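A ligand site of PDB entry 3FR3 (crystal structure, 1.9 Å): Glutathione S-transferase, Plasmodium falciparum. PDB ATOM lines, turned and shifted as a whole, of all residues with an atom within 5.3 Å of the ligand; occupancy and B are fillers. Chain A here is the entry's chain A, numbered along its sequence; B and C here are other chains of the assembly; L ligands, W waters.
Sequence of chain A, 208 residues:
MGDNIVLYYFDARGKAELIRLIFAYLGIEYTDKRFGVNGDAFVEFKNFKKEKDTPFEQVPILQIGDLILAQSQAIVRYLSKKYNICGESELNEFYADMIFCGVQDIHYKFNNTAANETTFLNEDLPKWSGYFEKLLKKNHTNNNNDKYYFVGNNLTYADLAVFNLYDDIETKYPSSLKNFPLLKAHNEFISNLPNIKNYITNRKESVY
Residues that only touch the ligand: Phe 10 (3.2 Å), Ala 12 (3.5 Å), Lys 15 (3.4 Å), Phe 45 (3.6 Å), Gln 58 (3.3 Å), Pro 60 (3.6 Å), Asn 116 of chain B (3.7 Å) and Glu 117 of chain B (3.6 Å). Of the 26 residues printed, 18 come within 4 Å of the ligand.
Water W10 lies within hydrogen-bond range of O of Glu 57 (2.6 Å), O5 of the ligand (2.7 Å), NZ of Lys 49 (2.9 Å) and OG1 of Thr 118 of chain B (3.0 Å). Water W9 lies within hydrogen-bond range of O of Pro 60 (2.6 Å), N of Gln 71 (2.9 Å) and O2 of the ligand (2.9 Å). Water W4 lies within hydrogen-bond range of the side-chain amide oxygen (OE1) of Gln 58 (2.7 Å) and an oxygen (O6) of the ligand (3.0 Å). Water W8 lies within hydrogen-bond range of N of Thr 119 of chain B (3.0 Å), O6 of the ligand (3.1 Å), N of Thr 118 of chain B (3.1 Å) and OE2 of Glu 117 of chain B (3.3 Å). Water W7 lies within hydrogen-bond range of the side-chain amide nitrogen of Gln 71 (3.0 Å), the backbone NH of Gln 73 (3.0 Å) and an oxygen (O1) of the ligand (3.2 Å). Water W5 lies within hydrogen-bond range of the backbone carbonyl oxygen of Cys 101 of chain C (2.7 Å), the side-chain carboxylate of Asp 105 of chain C (3.1 Å) and a nitrogen (N1) of the ligand (3.2 Å).
The backbone NH (N) of Lys 15 lies within hydrogen-bond range of the side-chain hydroxyl (OH) of Tyr 9 (3.0 Å). The side-chain hydroxyl (OG1) of Thr 118 of chain B sits at hydrogen-bond distance from the side-chain amino group (NZ) of Lys 49, 3.3 Å away. OD2 of Asp 105 of chain C lies close to OE1 of Gln 71. OD2 of Asp 105 of chain C sits at hydrogen-bond distance from NE2 of Gln 58, at 3.3 Å. The side-chain amide oxygen (OE1) of Gln 71 lies within hydrogen-bond range of the side-chain amide nitrogen (NE2) of Gln 58, at 3.2 Å.
N of Ser 72 is in hydrogen-bond range of O2 of the ligand (2.8 Å). OG of Ser 72 sits at hydrogen-bond distance from O1 of the ligand, at 2.5 Å. O12 of the ligand is in hydrogen-bond range of OH of Tyr 9 (2.5 Å). An oxygen (O5) of the ligand sits at hydrogen-bond distance from the backbone NH of Thr 118 of chain B (3.0 Å). O5 of the ligand lies within hydrogen-bond range of OG1 of Thr 118 of chain B, 2.6 Å away. The backbone NH (N) of Val 59 is in hydrogen-bond range of an oxygen (O4) of the ligand (3.0 Å). The backbone carbonyl oxygen of Val 59 sits at hydrogen-bond distance from a nitrogen (N2) of the ligand, 2.8 Å away. A nitrogen (N1) of the ligand lies within salt-bridge range of the side-chain carboxylate of Asp 105 of chain C (2.9 Å). N6 of the ligand sits close to N of Gly 14. The side-chain amide nitrogen of Gln 71 sits close to a nitrogen (N1) of the ligand, 2.9 Å away. The backbone NH (N) of Arg 13 sits at hydrogen-bond distance from an oxygen (O11) of the ligand, at 3.0 Å. An oxygen (O8) of the ligand is in salt-bridge range of the side-chain amino group (NZ) of Lys 172 of chain B (3.2 Å). The backbone NH of Ala 115 of chain B sits close to a sulfur (S2) of the ligand.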
ATOM      1  N   TYR A   9     -19.466 -20.612 -27.666  1.00  0.00           N
ATOM      2  CA  TYR A   9     -18.754 -19.364 -27.484  1.00  0.00           C
ATOM      3  C   TYR A   9     -17.284 -19.643 -27.704  1.00  0.00           C
ATOM      4  O   TYR A   9     -16.904 -20.783 -27.979  1.00  0.00           O
ATOM      5  CB  TYR A   9     -19.025 -18.821 -26.079  1.00  0.00           C
ATOM      6  CG  TYR A   9     -18.621 -17.401 -25.881  1.00  0.00           C
ATOM      7  CD1 TYR A   9     -17.609 -17.079 -24.976  1.00  0.00           C
ATOM      8  CD2 TYR A   9     -19.231 -16.373 -26.596  1.00  0.00           C
ATOM      9  CE1 TYR A   9     -17.228 -15.742 -24.757  1.00  0.00           C
ATOM     10  CE2 TYR A   9     -18.864 -15.035 -26.382  1.00  0.00           C
ATOM     11  CZ  TYR A   9     -17.871 -14.726 -25.486  1.00  0.00           C
ATOM     12  OH  TYR A   9     -17.523 -13.413 -25.300  1.00  0.00           O
ATOM     13  N   PHE A  10     -16.465 -18.592 -27.642  1.00  0.00           N
ATOM     14  CA  PHE A  10     -15.012 -18.739 -27.660  1.00  0.00           C
ATOM     15  C   PHE A  10     -14.582 -19.265 -26.294  1.00  0.00           C
ATOM     16  O   PHE A  10     -15.391 -19.377 -25.346  1.00  0.00           O
ATOM     17  CB  PHE A  10     -14.368 -17.381 -27.970  1.00  0.00           C
ATOM     18  CG  PHE A  10     -14.574 -16.949 -29.356  1.00  0.00           C
ATOM     19  CD1 PHE A  10     -15.537 -15.990 -29.657  1.00  0.00           C
ATOM     20  CD2 PHE A  10     -13.865 -17.568 -30.400  1.00  0.00           C
ATOM     21  CE1 PHE A  10     -15.752 -15.601 -30.985  1.00  0.00           C
ATOM     22  CE2 PHE A  10     -14.080 -17.191 -31.709  1.00  0.00           C
ATOM     23  CZ  PHE A  10     -15.045 -16.199 -32.004  1.00  0.00           C
ATOM     24  N   ASP A  11     -13.280 -19.537 -26.134  1.00  0.00           N
ATOM     25  CA  ASP A  11     -12.798 -20.103 -24.852  1.00  0.00           C
ATOM     26  C   ASP A  11     -12.502 -18.941 -23.906  1.00  0.00           C
ATOM     27  O   ASP A  11     -11.344 -18.537 -23.710  1.00  0.00           O
ATOM     28  CB  ASP A  11     -11.511 -20.922 -25.101  1.00  0.00           C
ATOM     29  CG  ASP A  11     -10.981 -21.622 -23.876  1.00  0.00           C
ATOM     30  OD1 ASP A  11      -9.758 -21.861 -23.856  1.00  0.00           O
ATOM     31  OD2 ASP A  11     -11.738 -21.962 -22.973  1.00  0.00           O
ATOM     32  N   ALA A  12     -13.566 -18.411 -23.328  1.00  0.00           N
ATOM     33  CA  ALA A  12     -13.528 -17.197 -22.554  1.00  0.00           C
ATOM     34  C   ALA A  12     -14.847 -17.118 -21.783  1.00  0.00           C
ATOM     35  O   ALA A  12     -15.841 -17.846 -22.072  1.00  0.00           O
ATOM     36  CB  ALA A  12     -13.385 -15.950 -23.473  1.00  0.00           C
ATOM     37  N   ARG A  13     -14.817 -16.266 -20.767  1.00  0.00           N
ATOM     38  CA  ARG A  13     -15.941 -16.010 -19.898  1.00  0.00           C
ATOM     39  C   ARG A  13     -16.812 -15.008 -20.649  1.00  0.00           C
ATOM     40  O   ARG A  13     -17.766 -15.414 -21.255  1.00  0.00           O
ATOM     41  CB  ARG A  13     -15.436 -15.428 -18.565  1.00  0.00           C
ATOM     42  CG  ARG A  13     -14.684 -16.546 -17.747  1.00  0.00           C
ATOM     43  CD  ARG A  13     -14.387 -16.164 -16.318  1.00  0.00           C
ATOM     44  NE  ARG A  13     -13.576 -17.246 -15.713  1.00  0.00           N
ATOM     45  CZ  ARG A  13     -13.030 -17.202 -14.502  1.00  0.00           C
ATOM     46  NH1 ARG A  13     -13.265 -16.163 -13.733  1.00  0.00           N
ATOM     47  NH2 ARG A  13     -12.315 -18.248 -14.050  1.00  0.00           N
ATOM     48  N   GLY A  14     -16.451 -13.723 -20.584  1.00  0.00           N
ATOM     49  CA  GLY A  14     -16.995 -12.708 -21.490  1.00  0.00           C
ATOM     50  C   GLY A  14     -18.508 -12.766 -21.544  1.00  0.00           C
ATOM     51  O   GLY A  14     -19.180 -12.763 -20.487  1.00  0.00           O
ATOM     52  N   LYS A  15     -19.041 -12.785 -22.787  1.00  0.00           N
ATOM     53  CA  LYS A  15     -20.457 -12.697 -23.054  1.00  0.00           C
ATOM     54  C   LYS A  15     -21.265 -13.986 -22.846  1.00  0.00           C
ATOM     55  O   LYS A  15     -22.510 -13.979 -22.935  1.00  0.00           O
ATOM     56  CB  LYS A  15     -20.692 -12.123 -24.463  1.00  0.00           C
ATOM     57  CG  LYS A  15     -20.253 -10.655 -24.582  1.00  0.00           C
ATOM     58  CD  LYS A  15     -20.235 -10.208 -26.080  1.00  0.00           C
ATOM     59  CE  LYS A  15     -19.342  -8.970 -26.360  1.00  0.00           C
ATOM     60  NZ  LYS A  15     -19.433  -7.986 -25.187  1.00  0.00           N
ATOM     61  N   PHE A  45     -14.457 -20.961 -35.436  1.00  0.00           N
ATOM     62  CA  PHE A  45     -15.628 -20.072 -35.500  1.00  0.00           C
ATOM     63  C   PHE A  45     -16.120 -19.905 -36.930  1.00  0.00           C
ATOM     64  O   PHE A  45     -17.298 -20.035 -37.213  1.00  0.00           O
ATOM     65  CB  PHE A  45     -15.241 -18.717 -34.953  1.00  0.00           C
ATOM     66  CG  PHE A  45     -16.378 -17.726 -34.970  1.00  0.00           C
ATOM     67  CD1 PHE A  45     -16.192 -16.437 -35.468  1.00  0.00           C
ATOM     68  CD2 PHE A  45     -17.649 -18.096 -34.505  1.00  0.00           C
ATOM     69  CE1 PHE A  45     -17.274 -15.515 -35.450  1.00  0.00           C
ATOM     70  CE2 PHE A  45     -18.709 -17.157 -34.503  1.00  0.00           C
ATOM     71  CZ  PHE A  45     -18.490 -15.893 -34.968  1.00  0.00           C
ATOM     72  N   LYS A  49     -19.787 -20.951 -38.390  1.00  0.00           N
ATOM     73  CA  LYS A  49     -20.767 -20.107 -39.064  1.00  0.00           C
ATOM     74  C   LYS A  49     -21.224 -20.745 -40.365  1.00  0.00           C
ATOM     75  O   LYS A  49     -22.377 -20.554 -40.782  1.00  0.00           O
ATOM     76  CB  LYS A  49     -20.212 -18.718 -39.347  1.00  0.00           C
ATOM     77  CG  LYS A  49     -20.053 -17.829 -38.144  1.00  0.00           C
ATOM     78  CD  LYS A  49     -19.496 -16.475 -38.559  1.00  0.00           C
ATOM     79  CE  LYS A  49     -18.001 -16.459 -38.840  1.00  0.00           C
ATOM     80  NZ  LYS A  49     -17.554 -15.133 -39.447  1.00  0.00           N
ATOM     81  N   GLU A  57     -23.993 -13.674 -37.211  1.00  0.00           N
ATOM     82  CA  GLU A  57     -22.574 -14.200 -37.268  1.00  0.00           C
ATOM     83  C   GLU A  57     -21.744 -13.859 -36.045  1.00  0.00           C
ATOM     84  O   GLU A  57     -20.537 -13.579 -36.124  1.00  0.00           O
ATOM     85  CB  GLU A  57     -21.869 -13.743 -38.556  1.00  0.00           C
ATOM     86  CG  GLU A  57     -22.649 -14.238 -39.822  1.00  0.00           C
ATOM     87  CD  GLU A  57     -21.947 -13.862 -41.137  1.00  0.00           C
ATOM     88  OE1 GLU A  57     -21.727 -14.779 -41.947  1.00  0.00           O
ATOM     89  OE2 GLU A  57     -21.641 -12.677 -41.354  1.00  0.00           O
ATOM     90  N   GLN A  58     -22.399 -13.922 -34.881  1.00  0.00           N
ATOM     91  CA  GLN A  58     -21.778 -13.731 -33.598  1.00  0.00           C
ATOM     92  C   GLN A  58     -22.138 -14.859 -32.639  1.00  0.00           C
ATOM     93  O   GLN A  58     -23.123 -15.543 -32.822  1.00  0.00           O
ATOM     94  CB  GLN A  58     -22.239 -12.441 -32.879  1.00  0.00           C
ATOM     95  CG  GLN A  58     -22.135 -11.178 -33.745  1.00  0.00           C
ATOM     96  CD  GLN A  58     -22.835  -9.984 -33.059  1.00  0.00           C
ATOM     97  OE1 GLN A  58     -22.212  -8.921 -32.898  1.00  0.00           O
ATOM     98  NE2 GLN A  58     -24.058 -10.187 -32.546  1.00  0.00           N
ATOM     99  N   VAL A  59     -21.287 -15.006 -31.639  1.00  0.00           N
ATOM    100  CA  VAL A  59     -21.586 -15.824 -30.504  1.00  0.00           C
ATOM    101  C   VAL A  59     -21.635 -14.910 -29.264  1.00  0.00           C
ATOM    102  O   VAL A  59     -21.093 -13.830 -29.276  1.00  0.00           O
ATOM    103  CB  VAL A  59     -20.503 -16.932 -30.356  1.00  0.00           C
ATOM    104  CG1 VAL A  59     -20.761 -18.035 -31.466  1.00  0.00           C
ATOM    105  CG2 VAL A  59     -19.068 -16.323 -30.327  1.00  0.00           C
ATOM    106  N   PRO A  60     -22.248 -15.344 -28.176  1.00  0.00           N
ATOM    107  CA  PRO A  60     -22.841 -16.667 -27.951  1.00  0.00           C
ATOM    108  C   PRO A  60     -24.018 -17.020 -28.807  1.00  0.00           C
ATOM    109  O   PRO A  60     -24.846 -16.152 -29.190  1.00  0.00           O
ATOM    110  CB  PRO A  60     -23.305 -16.634 -26.479  1.00  0.00           C
ATOM    111  CG  PRO A  60     -23.405 -15.217 -26.124  1.00  0.00           C
ATOM    112  CD  PRO A  60     -22.347 -14.474 -26.982  1.00  0.00           C
ATOM    113  N   GLN A  71     -27.633 -13.552 -29.169  1.00  0.00           N
ATOM    114  CA  GLN A  71     -27.658 -12.260 -28.446  1.00  0.00           C
ATOM    115  C   GLN A  71     -27.692 -12.540 -27.003  1.00  0.00           C
ATOM    116  O   GLN A  71     -28.708 -12.920 -26.468  1.00  0.00           O
ATOM    117  CB  GLN A  71     -28.815 -11.290 -28.886  1.00  0.00           C
ATOM    118  CG  GLN A  71     -28.521 -10.661 -30.277  1.00  0.00           C
ATOM    119  CD  GLN A  71     -27.339  -9.651 -30.256  1.00  0.00           C
ATOM    120  OE1 GLN A  71     -26.810  -9.263 -31.311  1.00  0.00           O
ATOM    121  NE2 GLN A  71     -26.948  -9.217 -29.086  1.00  0.00           N
ATOM    122  N   SER A  72     -26.521 -12.491 -26.398  1.00  0.00           N
ATOM    123  CA  SER A  72     -26.401 -12.875 -24.992  1.00  0.00           C
ATOM    124  C   SER A  72     -27.462 -12.320 -24.042  1.00  0.00           C
ATOM    125  O   SER A  72     -27.965 -13.061 -23.206  1.00  0.00           O
ATOM    126  CB  SER A  72     -25.020 -12.488 -24.487  1.00  0.00           C
ATOM    127  OG  SER A  72     -24.830 -11.106 -24.381  1.00  0.00           O
ATOM    128  N   GLN A  73     -27.772 -11.029 -24.111  1.00  0.00           N
ATOM    129  CA  GLN A  73     -28.779 -10.445 -23.163  1.00  0.00           C
ATOM    130  C   GLN A  73     -30.136 -10.994 -23.377  1.00  0.00           C
ATOM    131  O   GLN A  73     -30.887 -11.171 -22.456  1.00  0.00           O
ATOM    132  CB  GLN A  73     -28.920  -8.942 -23.401  1.00  0.00           C
ATOM    133  CG  GLN A  73     -27.734  -8.205 -22.987  1.00  0.00           C
ATOM    134  CD  GLN A  73     -27.980  -6.664 -23.051  1.00  0.00           C
ATOM    135  OE1 GLN A  73     -27.026  -5.948 -23.319  1.00  0.00           O
ATOM    136  NE2 GLN A  73     -29.248  -6.171 -22.842  1.00  0.00           N
ATOM    137  N   ASP A 168     -15.360 -10.811 -11.917  1.00  0.00           N
ATOM    138  CA  ASP A 168     -14.400 -10.410 -13.009  1.00  0.00           C
ATOM    139  C   ASP A 168     -13.513  -9.269 -12.478  1.00  0.00           C
ATOM    140  O   ASP A 168     -12.297  -9.348 -12.572  1.00  0.00           O
ATOM    141  CB  ASP A 168     -15.191  -9.925 -14.267  1.00  0.00           C
ATOM    142  CG  ASP A 168     -14.393  -9.989 -15.585  1.00  0.00           C
ATOM    143  OD1 ASP A 168     -13.192 -10.359 -15.582  1.00  0.00           O
ATOM    144  OD2 ASP A 168     -14.967  -9.647 -16.645  1.00  0.00           O
ATOM    145  N   ALA B 114     -11.473  -6.572 -30.587  1.00  0.00           N
ATOM    146  CA  ALA B 114     -11.670  -7.854 -29.918  1.00  0.00           C
ATOM    147  C   ALA B 114     -12.958  -8.597 -30.255  1.00  0.00           C
ATOM    148  O   ALA B 114     -14.061  -7.992 -30.364  1.00  0.00           O
ATOM    149  CB  ALA B 114     -11.556  -7.696 -28.380  1.00  0.00           C
ATOM    150  N   ALA B 115     -12.809  -9.904 -30.456  1.00  0.00           N
ATOM    151  CA  ALA B 115     -11.482 -10.548 -30.673  1.00  0.00           C
ATOM    152  C   ALA B 115     -11.829 -11.670 -31.608  1.00  0.00           C
ATOM    153  O   ALA B 115     -12.944 -12.235 -31.525  1.00  0.00           O
ATOM    154  CB  ALA B 115     -10.833 -11.079 -29.389  1.00  0.00           C
ATOM    155  N   ASN B 116     -10.860 -11.998 -32.456  1.00  0.00           N
ATOM    156  CA  ASN B 116     -11.093 -12.432 -33.835  1.00  0.00           C
ATOM    157  C   ASN B 116     -12.332 -11.836 -34.509  1.00  0.00           C
ATOM    158  O   ASN B 116     -13.240 -12.565 -34.981  1.00  0.00           O
ATOM    159  CB  ASN B 116     -10.926 -13.943 -34.037  1.00  0.00           C
ATOM    160  CG  ASN B 116     -11.897 -14.783 -33.238  1.00  0.00           C
ATOM    161  OD1 ASN B 116     -12.102 -14.568 -32.036  1.00  0.00           O
ATOM    162  ND2 ASN B 116     -12.472 -15.788 -33.891  1.00  0.00           N
ATOM    163  N   GLU B 117     -12.384 -10.510 -34.537  1.00  0.00           N
ATOM    164  CA  GLU B 117     -13.378  -9.755 -35.287  1.00  0.00           C
ATOM    165  C   GLU B 117     -13.129 -10.003 -36.753  1.00  0.00           C
ATOM    166  O   GLU B 117     -11.998  -9.851 -37.231  1.00  0.00           O
ATOM    167  CB  GLU B 117     -13.208  -8.285 -35.025  1.00  0.00           C
ATOM    168  CG  GLU B 117     -14.253  -7.389 -35.637  1.00  0.00           C
ATOM    169  CD  GLU B 117     -15.330  -7.028 -34.628  1.00  0.00           C
ATOM    170  OE1 GLU B 117     -15.187  -7.433 -33.456  1.00  0.00           O
ATOM    171  OE2 GLU B 117     -16.296  -6.337 -34.990  1.00  0.00           O
ATOM    172  N   THR B 118     -14.197 -10.393 -37.451  1.00  0.00           N
ATOM    173  CA  THR B 118     -14.161 -10.747 -38.833  1.00  0.00           C
ATOM    174  C   THR B 118     -13.851  -9.527 -39.694  1.00  0.00           C
ATOM    175  O   THR B 118     -13.152  -9.640 -40.685  1.00  0.00           O
ATOM    176  CB  THR B 118     -15.532 -11.364 -39.174  1.00  0.00           C
ATOM    177  OG1 THR B 118     -15.640 -12.597 -38.465  1.00  0.00           O
ATOM    178  CG2 THR B 118     -15.712 -11.598 -40.627  1.00  0.00           C
ATOM    179  N   THR B 119     -14.397  -8.381 -39.314  1.00  0.00           N
ATOM    180  CA  THR B 119     -14.226  -7.139 -40.064  1.00  0.00           C
ATOM    181  C   THR B 119     -12.748  -6.747 -40.007  1.00  0.00           C
ATOM    182  O   THR B 119     -12.166  -6.396 -41.022  1.00  0.00           O
ATOM    183  CB  THR B 119     -15.120  -6.007 -39.517  1.00  0.00           C
ATOM    184  OG1 THR B 119     -16.506  -6.360 -39.741  1.00  0.00           O
ATOM    185  CG2 THR B 119     -14.836  -4.683 -40.212  1.00  0.00           C
ATOM    186  N   LYS B 172      -1.284 -13.672 -32.685  1.00  0.00           N
ATOM    187  CA  LYS B 172      -2.717 -13.922 -32.582  1.00  0.00           C
ATOM    188  C   LYS B 172      -3.224 -14.508 -33.891  1.00  0.00           C
ATOM    189  O   LYS B 172      -4.001 -15.452 -33.909  1.00  0.00           O
ATOM    190  CB  LYS B 172      -3.443 -12.645 -32.126  1.00  0.00           C
ATOM    191  CG  LYS B 172      -4.940 -12.769 -32.036  1.00  0.00           C
ATOM    192  CD  LYS B 172      -5.493 -12.196 -30.763  1.00  0.00           C
ATOM    193  CE  LYS B 172      -6.897 -12.778 -30.521  1.00  0.00           C
ATOM    194  NZ  LYS B 172      -7.241 -12.914 -29.075  1.00  0.00           N
ATOM    195  N   CYS C 101     -31.411  -6.270 -29.684  1.00  0.00           N
ATOM    196  CA  CYS C 101     -30.034  -6.356 -29.270  1.00  0.00           C
ATOM    197  C   CYS C 101     -29.074  -6.232 -30.466  1.00  0.00           C
ATOM    198  O   CYS C 101     -27.991  -5.624 -30.349  1.00  0.00           O
ATOM    199  CB  CYS C 101     -29.807  -7.696 -28.534  1.00  0.00           C
ATOM    200  SG  CYS C 101     -30.604  -7.724 -26.891  1.00  0.00           S
ATOM    201  N   ASP C 105     -25.995  -3.353 -31.401  1.00  0.00           N
ATOM    202  CA  ASP C 105     -24.610  -3.602 -31.870  1.00  0.00           C
ATOM    203  C   ASP C 105     -24.296  -2.705 -33.060  1.00  0.00           C
ATOM    204  O   ASP C 105     -23.276  -2.007 -33.050  1.00  0.00           O
ATOM    205  CB  ASP C 105     -24.439  -5.094 -32.302  1.00  0.00           C
ATOM    206  CG  ASP C 105     -24.329  -6.039 -31.114  1.00  0.00           C
ATOM    207  OD1 ASP C 105     -24.069  -5.582 -29.962  1.00  0.00           O
ATOM    208  OD2 ASP C 105     -24.594  -7.204 -31.319  1.00  0.00           O
HETATM  209  N1  LIG L   1     -24.299  -8.104 -28.616  1.00  0.00           N
HETATM  210  C1  LIG L   1     -23.843  -9.460 -28.868  1.00  0.00           C
HETATM  211  C2  LIG L   1     -24.087 -10.372 -27.662  1.00  0.00           C
HETATM  212  O1  LIG L   1     -24.054  -9.938 -26.500  1.00  0.00           O
HETATM  213  O2  LIG L   1     -24.309 -11.603 -27.824  1.00  0.00           O
HETATM  214  C3  LIG L   1     -22.362  -9.333 -29.210  1.00  0.00           C
HETATM  215  C4  LIG L   1     -21.705 -10.700 -29.340  1.00  0.00           C
HETATM  216  C5  LIG L   1     -20.243 -10.524 -29.745  1.00  0.00           C
HETATM  217  O3  LIG L   1     -19.704  -9.436 -29.751  1.00  0.00           O
HETATM  218  N2  LIG L   1     -19.580 -11.657 -30.057  1.00  0.00           N
HETATM  219  C6  LIG L   1     -18.225 -11.649 -30.516  1.00  0.00           C
HETATM  220  C7  LIG L   1     -18.303 -12.212 -31.894  1.00  0.00           C
HETATM  221  O4  LIG L   1     -18.926 -13.214 -32.110  1.00  0.00           O
HETATM  222  C8  LIG L   1     -17.289 -12.552 -29.737  1.00  0.00           C
HETATM  223  S1  LIG L   1     -17.223 -12.208 -28.016  1.00  0.00           S
HETATM  224  N3  LIG L   1     -17.637 -11.571 -32.806  1.00  0.00           N
HETATM  225  C9  LIG L   1     -17.262 -12.237 -34.055  1.00  0.00           C
HETATM  226  C10 LIG L   1     -17.066 -11.241 -35.131  1.00  0.00           C
HETATM  227  O5  LIG L   1     -16.697 -11.613 -36.265  1.00  0.00           O
HETATM  228  O6  LIG L   1     -17.277 -10.050 -34.820  1.00  0.00           O
HETATM  229  N4  LIG L   1     -11.912 -14.367 -26.300  1.00  0.00           N
HETATM  230  C11 LIG L   1     -11.137 -15.594 -26.421  1.00  0.00           C
HETATM  231  C12 LIG L   1      -9.666 -15.423 -26.685  1.00  0.00           C
HETATM  232  O7  LIG L   1      -8.943 -16.448 -26.650  1.00  0.00           O
HETATM  233  O8  LIG L   1      -9.211 -14.276 -26.927  1.00  0.00           O
HETATM  234  C13 LIG L   1     -12.750 -13.979 -27.284  1.00  0.00           C
HETATM  235  O9  LIG L   1     -12.713 -14.466 -28.411  1.00  0.00           O
HETATM  236  C14 LIG L   1     -13.781 -12.904 -26.991  1.00  0.00           C
HETATM  237  N5  LIG L   1     -13.537 -12.076 -25.790  1.00  0.00           N
HETATM  238  C15 LIG L   1     -14.042 -12.127 -28.308  1.00  0.00           C
HETATM  239  S2  LIG L   1     -15.524 -11.108 -28.239  1.00  0.00           S
HETATM  240  C16 LIG L   1     -13.556 -12.905 -20.955  1.00  0.00           C
HETATM  241  C17 LIG L   1     -12.464 -13.570 -20.150  1.00  0.00           C
HETATM  242  O10 LIG L   1     -11.863 -12.823 -19.319  1.00  0.00           O
HETATM  243  O11 LIG L   1     -12.204 -14.811 -20.251  1.00  0.00           O
HETATM  244  N6  LIG L   1     -14.174 -12.085 -19.932  1.00  0.00           N
HETATM  245  C18 LIG L   1     -13.005 -12.205 -22.248  1.00  0.00           C
HETATM  246  C19 LIG L   1     -13.834 -11.477 -23.348  1.00  0.00           C
HETATM  247  C20 LIG L   1     -14.202 -12.258 -24.620  1.00  0.00           C
HETATM  248  O12 LIG L   1     -15.126 -13.045 -24.528  1.00  0.00           O
HETATM  249  O   HOH W   1     -22.797  -6.866 -26.386  1.00  0.00           O
HETATM  250  O   HOH W   2     -11.280  -9.906 -26.224  1.00  0.00           O
HETATM  251  O   HOH W   3     -15.714 -11.818 -17.740  1.00  0.00           O
HETATM  252  O   HOH W   4     -19.661  -8.560 -33.829  1.00  0.00           O
HETATM  253  O   HOH W   5     -26.503  -5.877 -28.115  1.00  0.00           O
HETATM  254  O   HOH W   6     -10.617 -13.957 -23.586  1.00  0.00           O
HETATM  255  O   HOH W   7     -27.062  -9.009 -26.145  1.00  0.00           O
HETATM  256  O   HOH W   8     -16.711  -8.557 -37.444  1.00  0.00           O
HETATM  257  O   HOH W   9     -24.813 -13.623 -29.855  1.00  0.00           O
HETATM  258  O   HOH W  10     -18.479 -12.989 -37.670  1.00  0.00           O
